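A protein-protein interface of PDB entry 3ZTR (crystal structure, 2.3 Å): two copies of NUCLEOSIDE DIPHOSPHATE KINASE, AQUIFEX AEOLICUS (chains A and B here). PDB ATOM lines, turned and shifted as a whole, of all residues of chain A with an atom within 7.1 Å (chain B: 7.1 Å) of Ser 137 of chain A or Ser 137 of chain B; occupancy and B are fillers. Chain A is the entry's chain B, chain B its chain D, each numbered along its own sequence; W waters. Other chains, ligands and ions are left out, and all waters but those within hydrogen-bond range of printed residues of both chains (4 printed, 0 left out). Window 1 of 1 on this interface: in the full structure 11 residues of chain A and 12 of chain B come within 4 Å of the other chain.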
ATOM      1  N   ALA A  36      12.233 -17.588 -22.847  1.00  0.00           N
ATOM      2  CA  ALA A  36      13.579 -18.024 -22.498  1.00  0.00           C
ATOM      3  C   ALA A  36      14.535 -17.034 -23.141  1.00  0.00           C
ATOM      4  O   ALA A  36      14.204 -16.414 -24.152  1.00  0.00           O
ATOM      5  CB  ALA A  36      13.860 -19.468 -23.022  1.00  0.00           C
ATOM      6  N   LYS A  38      19.022 -16.302 -23.329  1.00  0.00           N
ATOM      7  CA  LYS A  38      20.369 -16.376 -22.823  1.00  0.00           C
ATOM      8  C   LYS A  38      21.467 -15.967 -23.819  1.00  0.00           C
ATOM      9  O   LYS A  38      21.321 -16.104 -25.037  1.00  0.00           O
ATOM     10  CB  LYS A  38      20.646 -17.761 -22.254  1.00  0.00           C
ATOM     11  CG  LYS A  38      21.133 -18.750 -23.223  1.00  0.00           C
ATOM     12  CD  LYS A  38      21.354 -20.094 -22.513  1.00  0.00           C
ATOM     13  CE  LYS A  38      21.107 -21.250 -23.491  1.00  0.00           C
ATOM     14  NZ  LYS A  38      21.061 -22.532 -22.711  1.00  0.00           N
ATOM     15  N   LYS A  46      28.865 -27.089 -32.583  1.00  0.00           N
ATOM     16  CA  LYS A  46      27.460 -26.916 -32.222  1.00  0.00           C
ATOM     17  C   LYS A  46      26.708 -26.089 -33.265  1.00  0.00           C
ATOM     18  O   LYS A  46      25.562 -26.401 -33.603  1.00  0.00           O
ATOM     19  CB  LYS A  46      27.328 -26.272 -30.845  1.00  0.00           C
ATOM     20  CG  LYS A  46      27.756 -27.185 -29.719  1.00  0.00           C
ATOM     21  CD  LYS A  46      26.766 -28.303 -29.572  1.00  0.00           C
ATOM     22  CE  LYS A  46      27.106 -29.168 -28.377  1.00  0.00           C
ATOM     23  NZ  LYS A  46      26.280 -30.371 -28.444  1.00  0.00           N
ATOM     24  N   ILE A 132      14.525 -24.760 -30.804  1.00  0.00           N
ATOM     25  CA  ILE A 132      14.281 -24.375 -29.411  1.00  0.00           C
ATOM     26  C   ILE A 132      14.954 -25.392 -28.495  1.00  0.00           C
ATOM     27  O   ILE A 132      15.669 -25.023 -27.566  1.00  0.00           O
ATOM     28  CB  ILE A 132      12.768 -24.228 -29.126  1.00  0.00           C
ATOM     29  CG1 ILE A 132      12.237 -22.965 -29.836  1.00  0.00           C
ATOM     30  CG2 ILE A 132      12.458 -24.241 -27.591  1.00  0.00           C
ATOM     31  CD1 ILE A 132      10.693 -22.852 -29.854  1.00  0.00           C
ATOM     32  N   CYS A 133      14.757 -26.673 -28.782  1.00  0.00           N
ATOM     33  CA  CYS A 133      15.349 -27.735 -27.955  1.00  0.00           C
ATOM     34  C   CYS A 133      16.873 -27.771 -28.030  1.00  0.00           C
ATOM     35  O   CYS A 133      17.547 -28.168 -27.070  1.00  0.00           O
ATOM     36  CB  CYS A 133      14.778 -29.113 -28.317  1.00  0.00           C
ATOM     37  SG  CYS A 133      13.101 -29.369 -27.735  1.00  0.00           S
ATOM     38  N   PHE A 134      17.415 -27.365 -29.172  1.00  0.00           N
ATOM     39  CA  PHE A 134      18.858 -27.312 -29.328  1.00  0.00           C
ATOM     40  C   PHE A 134      19.491 -26.315 -28.359  1.00  0.00           C
ATOM     41  O   PHE A 134      20.580 -26.559 -27.836  1.00  0.00           O
ATOM     42  CB  PHE A 134      19.269 -26.964 -30.771  1.00  0.00           C
ATOM     43  CG  PHE A 134      20.681 -27.380 -31.084  1.00  0.00           C
ATOM     44  CD1 PHE A 134      20.951 -28.668 -31.524  1.00  0.00           C
ATOM     45  CD2 PHE A 134      21.731 -26.510 -30.875  1.00  0.00           C
ATOM     46  CE1 PHE A 134      22.261 -29.071 -31.775  1.00  0.00           C
ATOM     47  CE2 PHE A 134      23.039 -26.898 -31.129  1.00  0.00           C
ATOM     48  CZ  PHE A 134      23.308 -28.183 -31.581  1.00  0.00           C
ATOM     49  N   ILE A 135      18.807 -25.197 -28.130  1.00  0.00           N
ATOM     50  CA  ILE A 135      19.348 -24.095 -27.330  1.00  0.00           C
ATOM     51  C   ILE A 135      18.867 -24.090 -25.867  1.00  0.00           C
ATOM     52  O   ILE A 135      19.643 -23.813 -24.964  1.00  0.00           O
ATOM     53  CB  ILE A 135      19.024 -22.711 -27.988  1.00  0.00           C
ATOM     54  CG1 ILE A 135      19.604 -22.629 -29.413  1.00  0.00           C
ATOM     55  CG2 ILE A 135      19.511 -21.538 -27.098  1.00  0.00           C
ATOM     56  CD1 ILE A 135      21.095 -22.963 -29.499  1.00  0.00           C
ATOM     57  N   PHE A 136      17.603 -24.428 -25.644  1.00  0.00           N
ATOM     58  CA  PHE A 136      16.967 -24.309 -24.326  1.00  0.00           C
ATOM     59  C   PHE A 136      16.262 -25.618 -23.920  1.00  0.00           C
ATOM     60  O   PHE A 136      15.533 -26.216 -24.739  1.00  0.00           O
ATOM     61  CB  PHE A 136      15.876 -23.235 -24.384  1.00  0.00           C
ATOM     62  CG  PHE A 136      16.382 -21.840 -24.587  1.00  0.00           C
ATOM     63  CD1 PHE A 136      16.979 -21.140 -23.530  1.00  0.00           C
ATOM     64  CD2 PHE A 136      16.200 -21.194 -25.808  1.00  0.00           C
ATOM     65  CE1 PHE A 136      17.434 -19.817 -23.704  1.00  0.00           C
ATOM     66  CE2 PHE A 136      16.624 -19.873 -25.988  1.00  0.00           C
ATOM     67  CZ  PHE A 136      17.248 -19.178 -24.936  1.00  0.00           C
ATOM     68  N   SER A 137      16.461 -26.061 -22.674  1.00  0.00           N
ATOM     69  CA  SER A 137      15.663 -27.165 -22.137  1.00  0.00           C
ATOM     70  C   SER A 137      14.319 -26.648 -21.645  1.00  0.00           C
ATOM     71  O   SER A 137      14.118 -25.438 -21.524  1.00  0.00           O
ATOM     72  CB  SER A 137      16.357 -27.885 -20.969  1.00  0.00           C
ATOM     73  OG  SER A 137      16.392 -27.059 -19.818  1.00  0.00           O
ATOM     74  N   GLY A 138      13.407 -27.567 -21.352  1.00  0.00           N
ATOM     75  CA  GLY A 138      12.167 -27.201 -20.701  1.00  0.00           C
ATOM     76  C   GLY A 138      12.393 -26.503 -19.355  1.00  0.00           C
ATOM     77  O   GLY A 138      11.594 -25.648 -18.976  1.00  0.00           O
ATOM     78  N   LEU A 139      13.477 -26.846 -18.653  1.00  0.00           N
ATOM     79  CA  LEU A 139      13.848 -26.180 -17.402  1.00  0.00           C
ATOM     80  C   LEU A 139      14.141 -24.691 -17.585  1.00  0.00           C
ATOM     81  O   LEU A 139      13.962 -23.930 -16.641  1.00  0.00           O
ATOM     82  CB  LEU A 139      15.085 -26.853 -16.756  1.00  0.00           C
ATOM     83  CG  LEU A 139      14.850 -28.318 -16.393  1.00  0.00           C
ATOM     84  CD1 LEU A 139      16.139 -28.958 -15.857  1.00  0.00           C
ATOM     85  CD2 LEU A 139      13.702 -28.392 -15.396  1.00  0.00           C
ATOM     86  N   GLU A 140      14.585 -24.290 -18.783  1.00  0.00           N
ATOM     87  CA  GLU A 140      14.960 -22.885 -19.045  1.00  0.00           C
ATOM     88  C   GLU A 140      13.805 -22.014 -19.541  1.00  0.00           C
ATOM     89  O   GLU A 140      13.949 -20.807 -19.745  1.00  0.00           O
ATOM     90  CB  GLU A 140      16.107 -22.806 -20.058  1.00  0.00           C
ATOM     91  CG  GLU A 140      17.397 -23.407 -19.547  1.00  0.00           C
ATOM     92  CD  GLU A 140      18.446 -23.469 -20.635  1.00  0.00           C
ATOM     93  OE1 GLU A 140      19.179 -22.474 -20.810  1.00  0.00           O
ATOM     94  OE2 GLU A 140      18.531 -24.509 -21.326  1.00  0.00           O
ATOM     95  N   ILE A 141      12.677 -22.648 -19.787  1.00  0.00           N
ATOM     96  CA  ILE A 141      11.532 -21.940 -20.323  1.00  0.00           C
ATOM     97  C   ILE A 141      10.646 -21.587 -19.144  1.00  0.00           C
ATOM     98  O   ILE A 141      10.172 -22.472 -18.439  1.00  0.00           O
ATOM     99  CB  ILE A 141      10.810 -22.818 -21.345  1.00  0.00           C
ATOM    100  CG1 ILE A 141      11.720 -22.992 -22.560  1.00  0.00           C
ATOM    101  CG2 ILE A 141       9.494 -22.214 -21.731  1.00  0.00           C
ATOM    102  CD1 ILE A 141      11.231 -24.000 -23.577  1.00  0.00           C
ATOM    103  N   VAL A 142      10.472 -20.293 -18.896  1.00  0.00           N
ATOM    104  CA  VAL A 142       9.854 -19.857 -17.649  1.00  0.00           C
ATOM    105  C   VAL A 142       8.913 -18.692 -17.888  1.00  0.00           C
ATOM    106  O   VAL A 142       8.881 -18.127 -18.975  1.00  0.00           O
ATOM    107  CB  VAL A 142      10.922 -19.450 -16.612  1.00  0.00           C
ATOM    108  CG1 VAL A 142      11.809 -20.635 -16.262  1.00  0.00           C
ATOM    109  CG2 VAL A 142      11.756 -18.304 -17.137  1.00  0.00           C
ATOM    110  OXT VAL A 142       8.155 -18.292 -17.020  1.00  0.00           O
ATOM    111  N   ALA B  36      24.829 -36.649 -21.489  1.00  0.00           N
ATOM    112  CA  ALA B  36      24.523 -35.449 -20.717  1.00  0.00           C
ATOM    113  C   ALA B  36      24.256 -35.899 -19.297  1.00  0.00           C
ATOM    114  O   ALA B  36      23.820 -37.031 -19.080  1.00  0.00           O
ATOM    115  CB  ALA B  36      23.302 -34.723 -21.265  1.00  0.00           C
ATOM    116  N   LYS B  38      23.332 -34.033 -15.220  1.00  0.00           N
ATOM    117  CA  LYS B  38      23.304 -32.937 -14.287  1.00  0.00           C
ATOM    118  C   LYS B  38      22.445 -33.193 -13.092  1.00  0.00           C
ATOM    119  O   LYS B  38      21.447 -33.893 -13.170  1.00  0.00           O
ATOM    120  CB  LYS B  38      22.890 -31.638 -14.986  1.00  0.00           C
ATOM    121  CG  LYS B  38      21.439 -31.327 -14.987  1.00  0.00           C
ATOM    122  CD  LYS B  38      21.188 -30.002 -15.727  1.00  0.00           C
ATOM    123  CE  LYS B  38      19.811 -30.013 -16.418  1.00  0.00           C
ATOM    124  NZ  LYS B  38      19.720 -28.960 -17.484  1.00  0.00           N
ATOM    125  N   LYS B  46       7.432 -27.759 -12.527  1.00  0.00           N
ATOM    126  CA  LYS B  46       8.200 -28.375 -13.605  1.00  0.00           C
ATOM    127  C   LYS B  46       8.018 -29.881 -13.598  1.00  0.00           C
ATOM    128  O   LYS B  46       7.900 -30.509 -14.657  1.00  0.00           O
ATOM    129  CB  LYS B  46       9.677 -28.013 -13.485  1.00  0.00           C
ATOM    130  CG  LYS B  46       9.993 -26.592 -13.885  1.00  0.00           C
ATOM    131  CD  LYS B  46       9.697 -26.359 -15.368  1.00  0.00           C
ATOM    132  CE  LYS B  46      10.056 -24.931 -15.762  1.00  0.00           C
ATOM    133  NZ  LYS B  46       9.397 -24.561 -17.027  1.00  0.00           N
ATOM    134  N   ILE B 132      13.959 -35.815 -22.874  1.00  0.00           N
ATOM    135  CA  ILE B 132      15.332 -35.382 -23.013  1.00  0.00           C
ATOM    136  C   ILE B 132      15.359 -33.859 -23.213  1.00  0.00           C
ATOM    137  O   ILE B 132      16.119 -33.134 -22.532  1.00  0.00           O
ATOM    138  CB  ILE B 132      16.005 -36.088 -24.189  1.00  0.00           C
ATOM    139  CG1 ILE B 132      16.356 -37.539 -23.821  1.00  0.00           C
ATOM    140  CG2 ILE B 132      17.269 -35.310 -24.627  1.00  0.00           C
ATOM    141  CD1 ILE B 132      16.782 -38.369 -25.044  1.00  0.00           C
ATOM    142  N   CYS B 133      14.516 -33.368 -24.124  1.00  0.00           N
ATOM    143  CA  CYS B 133      14.405 -31.933 -24.365  1.00  0.00           C
ATOM    144  C   CYS B 133      13.910 -31.165 -23.128  1.00  0.00           C
ATOM    145  O   CYS B 133      14.272 -29.991 -22.919  1.00  0.00           O
ATOM    146  CB  CYS B 133      13.498 -31.670 -25.585  1.00  0.00           C
ATOM    147  SG  CYS B 133      14.278 -32.030 -27.199  1.00  0.00           S
ATOM    148  N   PHE B 134      13.062 -31.809 -22.325  1.00  0.00           N
ATOM    149  CA  PHE B 134      12.569 -31.130 -21.126  1.00  0.00           C
ATOM    150  C   PHE B 134      13.722 -30.772 -20.170  1.00  0.00           C
ATOM    151  O   PHE B 134      13.719 -29.708 -19.541  1.00  0.00           O
ATOM    152  CB  PHE B 134      11.471 -31.939 -20.393  1.00  0.00           C
ATOM    153  CG  PHE B 134      10.645 -31.092 -19.464  1.00  0.00           C
ATOM    154  CD1 PHE B 134      11.076 -30.835 -18.167  1.00  0.00           C
ATOM    155  CD2 PHE B 134       9.475 -30.486 -19.909  1.00  0.00           C
ATOM    156  CE1 PHE B 134      10.333 -30.001 -17.311  1.00  0.00           C
ATOM    157  CE2 PHE B 134       8.731 -29.640 -19.064  1.00  0.00           C
ATOM    158  CZ  PHE B 134       9.154 -29.410 -17.762  1.00  0.00           C
ATOM    159  N   ILE B 135      14.718 -31.651 -20.100  1.00  0.00           N
ATOM    160  CA  ILE B 135      15.779 -31.543 -19.102  1.00  0.00           C
ATOM    161  C   ILE B 135      17.088 -30.982 -19.682  1.00  0.00           C
ATOM    162  O   ILE B 135      17.772 -30.183 -19.050  1.00  0.00           O
ATOM    163  CB  ILE B 135      16.089 -32.933 -18.450  1.00  0.00           C
ATOM    164  CG1 ILE B 135      14.870 -33.479 -17.690  1.00  0.00           C
ATOM    165  CG2 ILE B 135      17.277 -32.828 -17.502  1.00  0.00           C
ATOM    166  CD1 ILE B 135      14.275 -32.479 -16.741  1.00  0.00           C
ATOM    167  N   PHE B 136      17.432 -31.395 -20.891  1.00  0.00           N
ATOM    168  CA  PHE B 136      18.696 -30.998 -21.508  1.00  0.00           C
ATOM    169  C   PHE B 136      18.514 -30.341 -22.884  1.00  0.00           C
ATOM    170  O   PHE B 136      17.757 -30.847 -23.700  1.00  0.00           O
ATOM    171  CB  PHE B 136      19.546 -32.244 -21.725  1.00  0.00           C
ATOM    172  CG  PHE B 136      20.019 -32.892 -20.468  1.00  0.00           C
ATOM    173  CD1 PHE B 136      21.029 -32.307 -19.698  1.00  0.00           C
ATOM    174  CD2 PHE B 136      19.505 -34.121 -20.081  1.00  0.00           C
ATOM    175  CE1 PHE B 136      21.500 -32.943 -18.536  1.00  0.00           C
ATOM    176  CE2 PHE B 136      19.980 -34.767 -18.948  1.00  0.00           C
ATOM    177  CZ  PHE B 136      20.984 -34.183 -18.175  1.00  0.00           C
ATOM    178  N   SER B 137      19.212 -29.233 -23.137  1.00  0.00           N
ATOM    179  CA  SER B 137      19.260 -28.652 -24.464  1.00  0.00           C
ATOM    180  C   SER B 137      20.298 -29.373 -25.316  1.00  0.00           C
ATOM    181  O   SER B 137      21.127 -30.101 -24.800  1.00  0.00           O
ATOM    182  CB  SER B 137      19.611 -27.170 -24.402  1.00  0.00           C
ATOM    183  OG  SER B 137      21.001 -26.981 -24.173  1.00  0.00           O
ATOM    184  N   GLY B 138      20.264 -29.147 -26.622  1.00  0.00           N
ATOM    185  CA  GLY B 138      21.323 -29.638 -27.479  1.00  0.00           C
ATOM    186  C   GLY B 138      22.699 -29.150 -27.056  1.00  0.00           C
ATOM    187  O   GLY B 138      23.705 -29.851 -27.229  1.00  0.00           O
ATOM    188  N   LEU B 139      22.760 -27.955 -26.484  1.00  0.00           N
ATOM    189  CA  LEU B 139      24.030 -27.432 -25.978  1.00  0.00           C
ATOM    190  C   LEU B 139      24.619 -28.278 -24.827  1.00  0.00           C
ATOM    191  O   LEU B 139      25.834 -28.316 -24.636  1.00  0.00           O
ATOM    192  CB  LEU B 139      23.866 -25.979 -25.523  1.00  0.00           C
ATOM    193  CG  LEU B 139      23.503 -25.013 -26.655  1.00  0.00           C
ATOM    194  CD1 LEU B 139      23.111 -23.604 -26.096  1.00  0.00           C
ATOM    195  CD2 LEU B 139      24.660 -24.954 -27.682  1.00  0.00           C
ATOM    196  N   GLU B 140      23.769 -28.956 -24.060  1.00  0.00           N
ATOM    197  CA  GLU B 140      24.249 -29.743 -22.919  1.00  0.00           C
ATOM    198  C   GLU B 140      24.599 -31.186 -23.281  1.00  0.00           C
ATOM    199  O   GLU B 140      25.057 -31.954 -22.421  1.00  0.00           O
ATOM    200  CB  GLU B 140      23.226 -29.761 -21.793  1.00  0.00           C
ATOM    201  CG  GLU B 140      22.996 -28.443 -21.115  1.00  0.00           C
ATOM    202  CD  GLU B 140      21.710 -28.460 -20.251  1.00  0.00           C
ATOM    203  OE1 GLU B 140      20.610 -28.160 -20.774  1.00  0.00           O
ATOM    204  OE2 GLU B 140      21.797 -28.784 -19.052  1.00  0.00           O
ATOM    205  N   ILE B 141      24.357 -31.572 -24.531  1.00  0.00           N
ATOM    206  CA  ILE B 141      24.646 -32.939 -24.957  1.00  0.00           C
ATOM    207  C   ILE B 141      26.017 -32.918 -25.581  1.00  0.00           C
ATOM    208  O   ILE B 141      26.231 -32.241 -26.587  1.00  0.00           O
ATOM    209  CB  ILE B 141      23.674 -33.431 -26.025  1.00  0.00           C
ATOM    210  CG1 ILE B 141      22.243 -33.028 -25.673  1.00  0.00           C
ATOM    211  CG2 ILE B 141      23.823 -34.925 -26.253  1.00  0.00           C
ATOM    212  CD1 ILE B 141      21.546 -33.964 -24.814  1.00  0.00           C
ATOM    213  N   VAL B 142      26.961 -33.640 -24.982  1.00  0.00           N
ATOM    214  CA  VAL B 142      28.366 -33.527 -25.393  1.00  0.00           C
ATOM    215  C   VAL B 142      29.076 -34.872 -25.427  1.00  0.00           C
ATOM    216  O   VAL B 142      28.567 -35.878 -24.969  1.00  0.00           O
ATOM    217  CB  VAL B 142      29.180 -32.536 -24.474  1.00  0.00           C
ATOM    218  CG1 VAL B 142      28.673 -31.070 -24.623  1.00  0.00           C
ATOM    219  CG2 VAL B 142      29.151 -32.985 -23.012  1.00  0.00           C
ATOM    220  OXT VAL B 142      30.196 -34.992 -25.907  1.00  0.00           O
HETATM  221  O   HOH W   1      11.111 -32.309 -29.090  1.00  0.00           O
HETATM  222  O   HOH W   2      20.932 -25.295 -21.992  1.00  0.00           O
HETATM  223  O   HOH W   3      19.005 -26.706 -19.195  1.00  0.00           O
HETATM  224  O   HOH W   4      17.730 -31.316 -26.236  1.00  0.00           O
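Water W4 lies within hydrogen-bond range of O of Phe 136 of chain B, O of Cys 133 of chain A, N of Gly 138 of chain B and SG of Cys 133 of chain B. Water W2 lies within hydrogen-bond range of the side-chain carboxylate of Glu 140 of chain A, the side-chain hydroxyl of Ser 137 of chain B, the side-chain amino group of Lys 38 of chain A and the side-chain carboxylate of Glu 140 of chain B. Water W3 lies within hydrogen-bond range of OE1 of Glu 140 of chain B (2.7 Å), OG of Ser 137 of chain A (2.7 Å), NZ of Lys 38 of chain B (2.9 Å) and OE2 of Glu 140 of chain A (3.1 Å). Water W1 lies within hydrogen-bond range of SG of Cys 133 of chain B (3.7 Å) and SG of Cys 133 of chain A (3.8 Å).
Of the printed residues of chain B, Ile 135 of chain A touches Ser 137 (3.4 Å) and Leu 139 (3.7 Å). Of the printed residues of chain B, Ser 137 of chain A touches Cys 133 (3.2 Å), Phe 134 (3.5 Å), Ile 135 (3.3 Å), Phe 136 (3.7 Å) and Ser 137 (3.8 Å). Printed residues of chain B within 4 Å of Leu 139 of chain A: Lys 38, Phe 134 and Ile 135. Ala 36 of chain B touches none of the printed residues of chain A. Printed residues of chain A within 4 Å of Lys 46 of chain B: Gly 138 and Ile 141. Of the printed residues of chain A, Phe 134 of chain B touches Ser 137 (3.5 Å), Gly 138 (2.8 Å) and Leu 139 (3.0 Å). Printed residues of chain A within 4 Å of Ser 137 of chain B: Cys 133 (3.2 Å), Phe 134 (3.6 Å), Ile 135 (3.4 Å), Phe 136 (3.6 Å) and Ser 137 (3.8 Å). Printed residues of chain A within 4 Å of Ile 141 of chain B: Lys 46. The nearest printed residue of chain B that does not touch Ser 137 of chain A is Glu 140 of chain B (4.3 Å). The nearest printed residue of chain A that does not touch Ser 137 of chain B is Glu 140 of chain A (4.2 Å).
CA of Ser 137 of chain B touches O of Cys 133 of chain A, at 3.2 Å. Ser 137 of chain B touches Phe 134 of chain A (CB to O, 3.6 Å). Ile 135 of chain A touches Ser 137 of chain B. Ile 135 of chain A touches Leu 139 of chain B (O to CD1, 3.7 Å). Ser 137 of chain B touches Phe 136 of chain A. Ser 137 of chain A touches Phe 134 of chain B (CB to O, 3.5 Å). O of Ile 135 of chain B touches CB of Ser 137 of chain A (3.3 Å). Phe 136 of chain B touches Ser 137 of chain A (N to CB, 3.7 Å). Ser 137 of chain B touches Ser 137 of chain A (CB to N, 3.8 Å). Leu 139 of chain A touches Lys 38 of chain B (CD1 to CE, 3.9 Å).
Cys 133 of chain A touches Ser 137 of chain B, and with the chains exchanged Ser 137 of chain A touches Cys 133 of chain B. Phe 134 of chain A touches Gly 138 of chain B, and with the chains exchanged Gly 138 of chain A touches Phe 134 of chain B. Phe 134 of chain A touches Leu 139 of chain B, and with the chains exchanged Leu 139 of chain A touches Phe 134 of chain B. Ser 137 of chain A touches its own counterpart, Ser 137 of chain B. Positions printed for both chains: 36, 38, 46, 132, 133, 134, 135, 136, 137, 138, 139, 140, 141 and 142.
Hydrophobic or aromatic side chains of chain B within 4 Å of the printed part of chain A: Leu 139. Hydrophobic or aromatic side chains of chain A within 4 Å of the printed part of chain B: Leu 139. Among the printed residues, 23 pairs touch across the chains. Among the printed residues, no Asp or Glu carboxylate lies within 4 Å of a Lys or Arg side-chain nitrogen of the other chain.
The side-chain amino group (NZ) of Lys 46 of chain A sits at hydrogen-bond distance from the backbone carbonyl oxygen (O) of Gly 138 of chain B (2.9 Å). The backbone NH (N) of Leu 139 of chain B is in hydrogen-bond range of the backbone carbonyl oxygen (O) of Phe 134 of chain A (2.9 Å). The backbone carbonyl oxygen (O) of Cys 133 of chain B lies within hydrogen-bond range of the backbone NH (N) of Gly 138 of chain A (3.0 Å). The backbone carbonyl oxygen of Gly 138 of chain A sits at hydrogen-bond distance from the side-chain amino group of Lys 46 of chain B (3.1 Å). The backbone NH of Gly 138 of chain A lies within hydrogen-bond range of the backbone carbonyl oxygen of Phe 134 of chain B, 2.8 Å away. SG of Cys 133 of chain A lies close to SG of Cys 133 of chain B, at 3.0 Å. N of Leu 139 of chain A is in hydrogen-bond range of O of Phe 134 of chain B, 3.0 Å away. O of Phe 134 of chain A is in hydrogen-bond range of N of Gly 138 of chain B, 2.9 Å away. The backbone NH (N) of Gly 138 of chain B lies within hydrogen-bond range of the backbone carbonyl oxygen (O) of Cys 133 of chain A (2.9 Å). NZ of Lys 46 of chain A lies within hydrogen-bond range of O of Ile 141 of chain B. The side-chain amino group of Lys 46 of chain B is in hydrogen-bond range of the backbone carbonyl oxygen of Ile 141 of chain A, 2.6 Å away.
OG of Ser 137 of chain B is in hydrogen-bond range of N of Leu 139 of chain B, at 3.1 Å. The backbone NH (N) of Leu 139 of chain A sits close to the side-chain hydroxyl (OG) of Ser 137 of chain A (3.1 Å). The side-chain amino group (NZ) of Lys 38 of chain A is in hydrogen-bond range of the backbone carbonyl oxygen (O) of Ile 135 of chain A, at 3.0 Å. The side-chain amino group (NZ) of Lys 38 of chain B is in salt-bridge range of the side-chain carboxylate (OE2) of Glu 140 of chain B, 2.6 Å away. N of Ser 137 of chain B is in hydrogen-bond range of OE1 of Glu 140 of chain B (2.9 Å). The backbone NH of Ser 137 of chain A is in hydrogen-bond range of the side-chain carboxylate of Glu 140 of chain A, at 2.9 Å.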
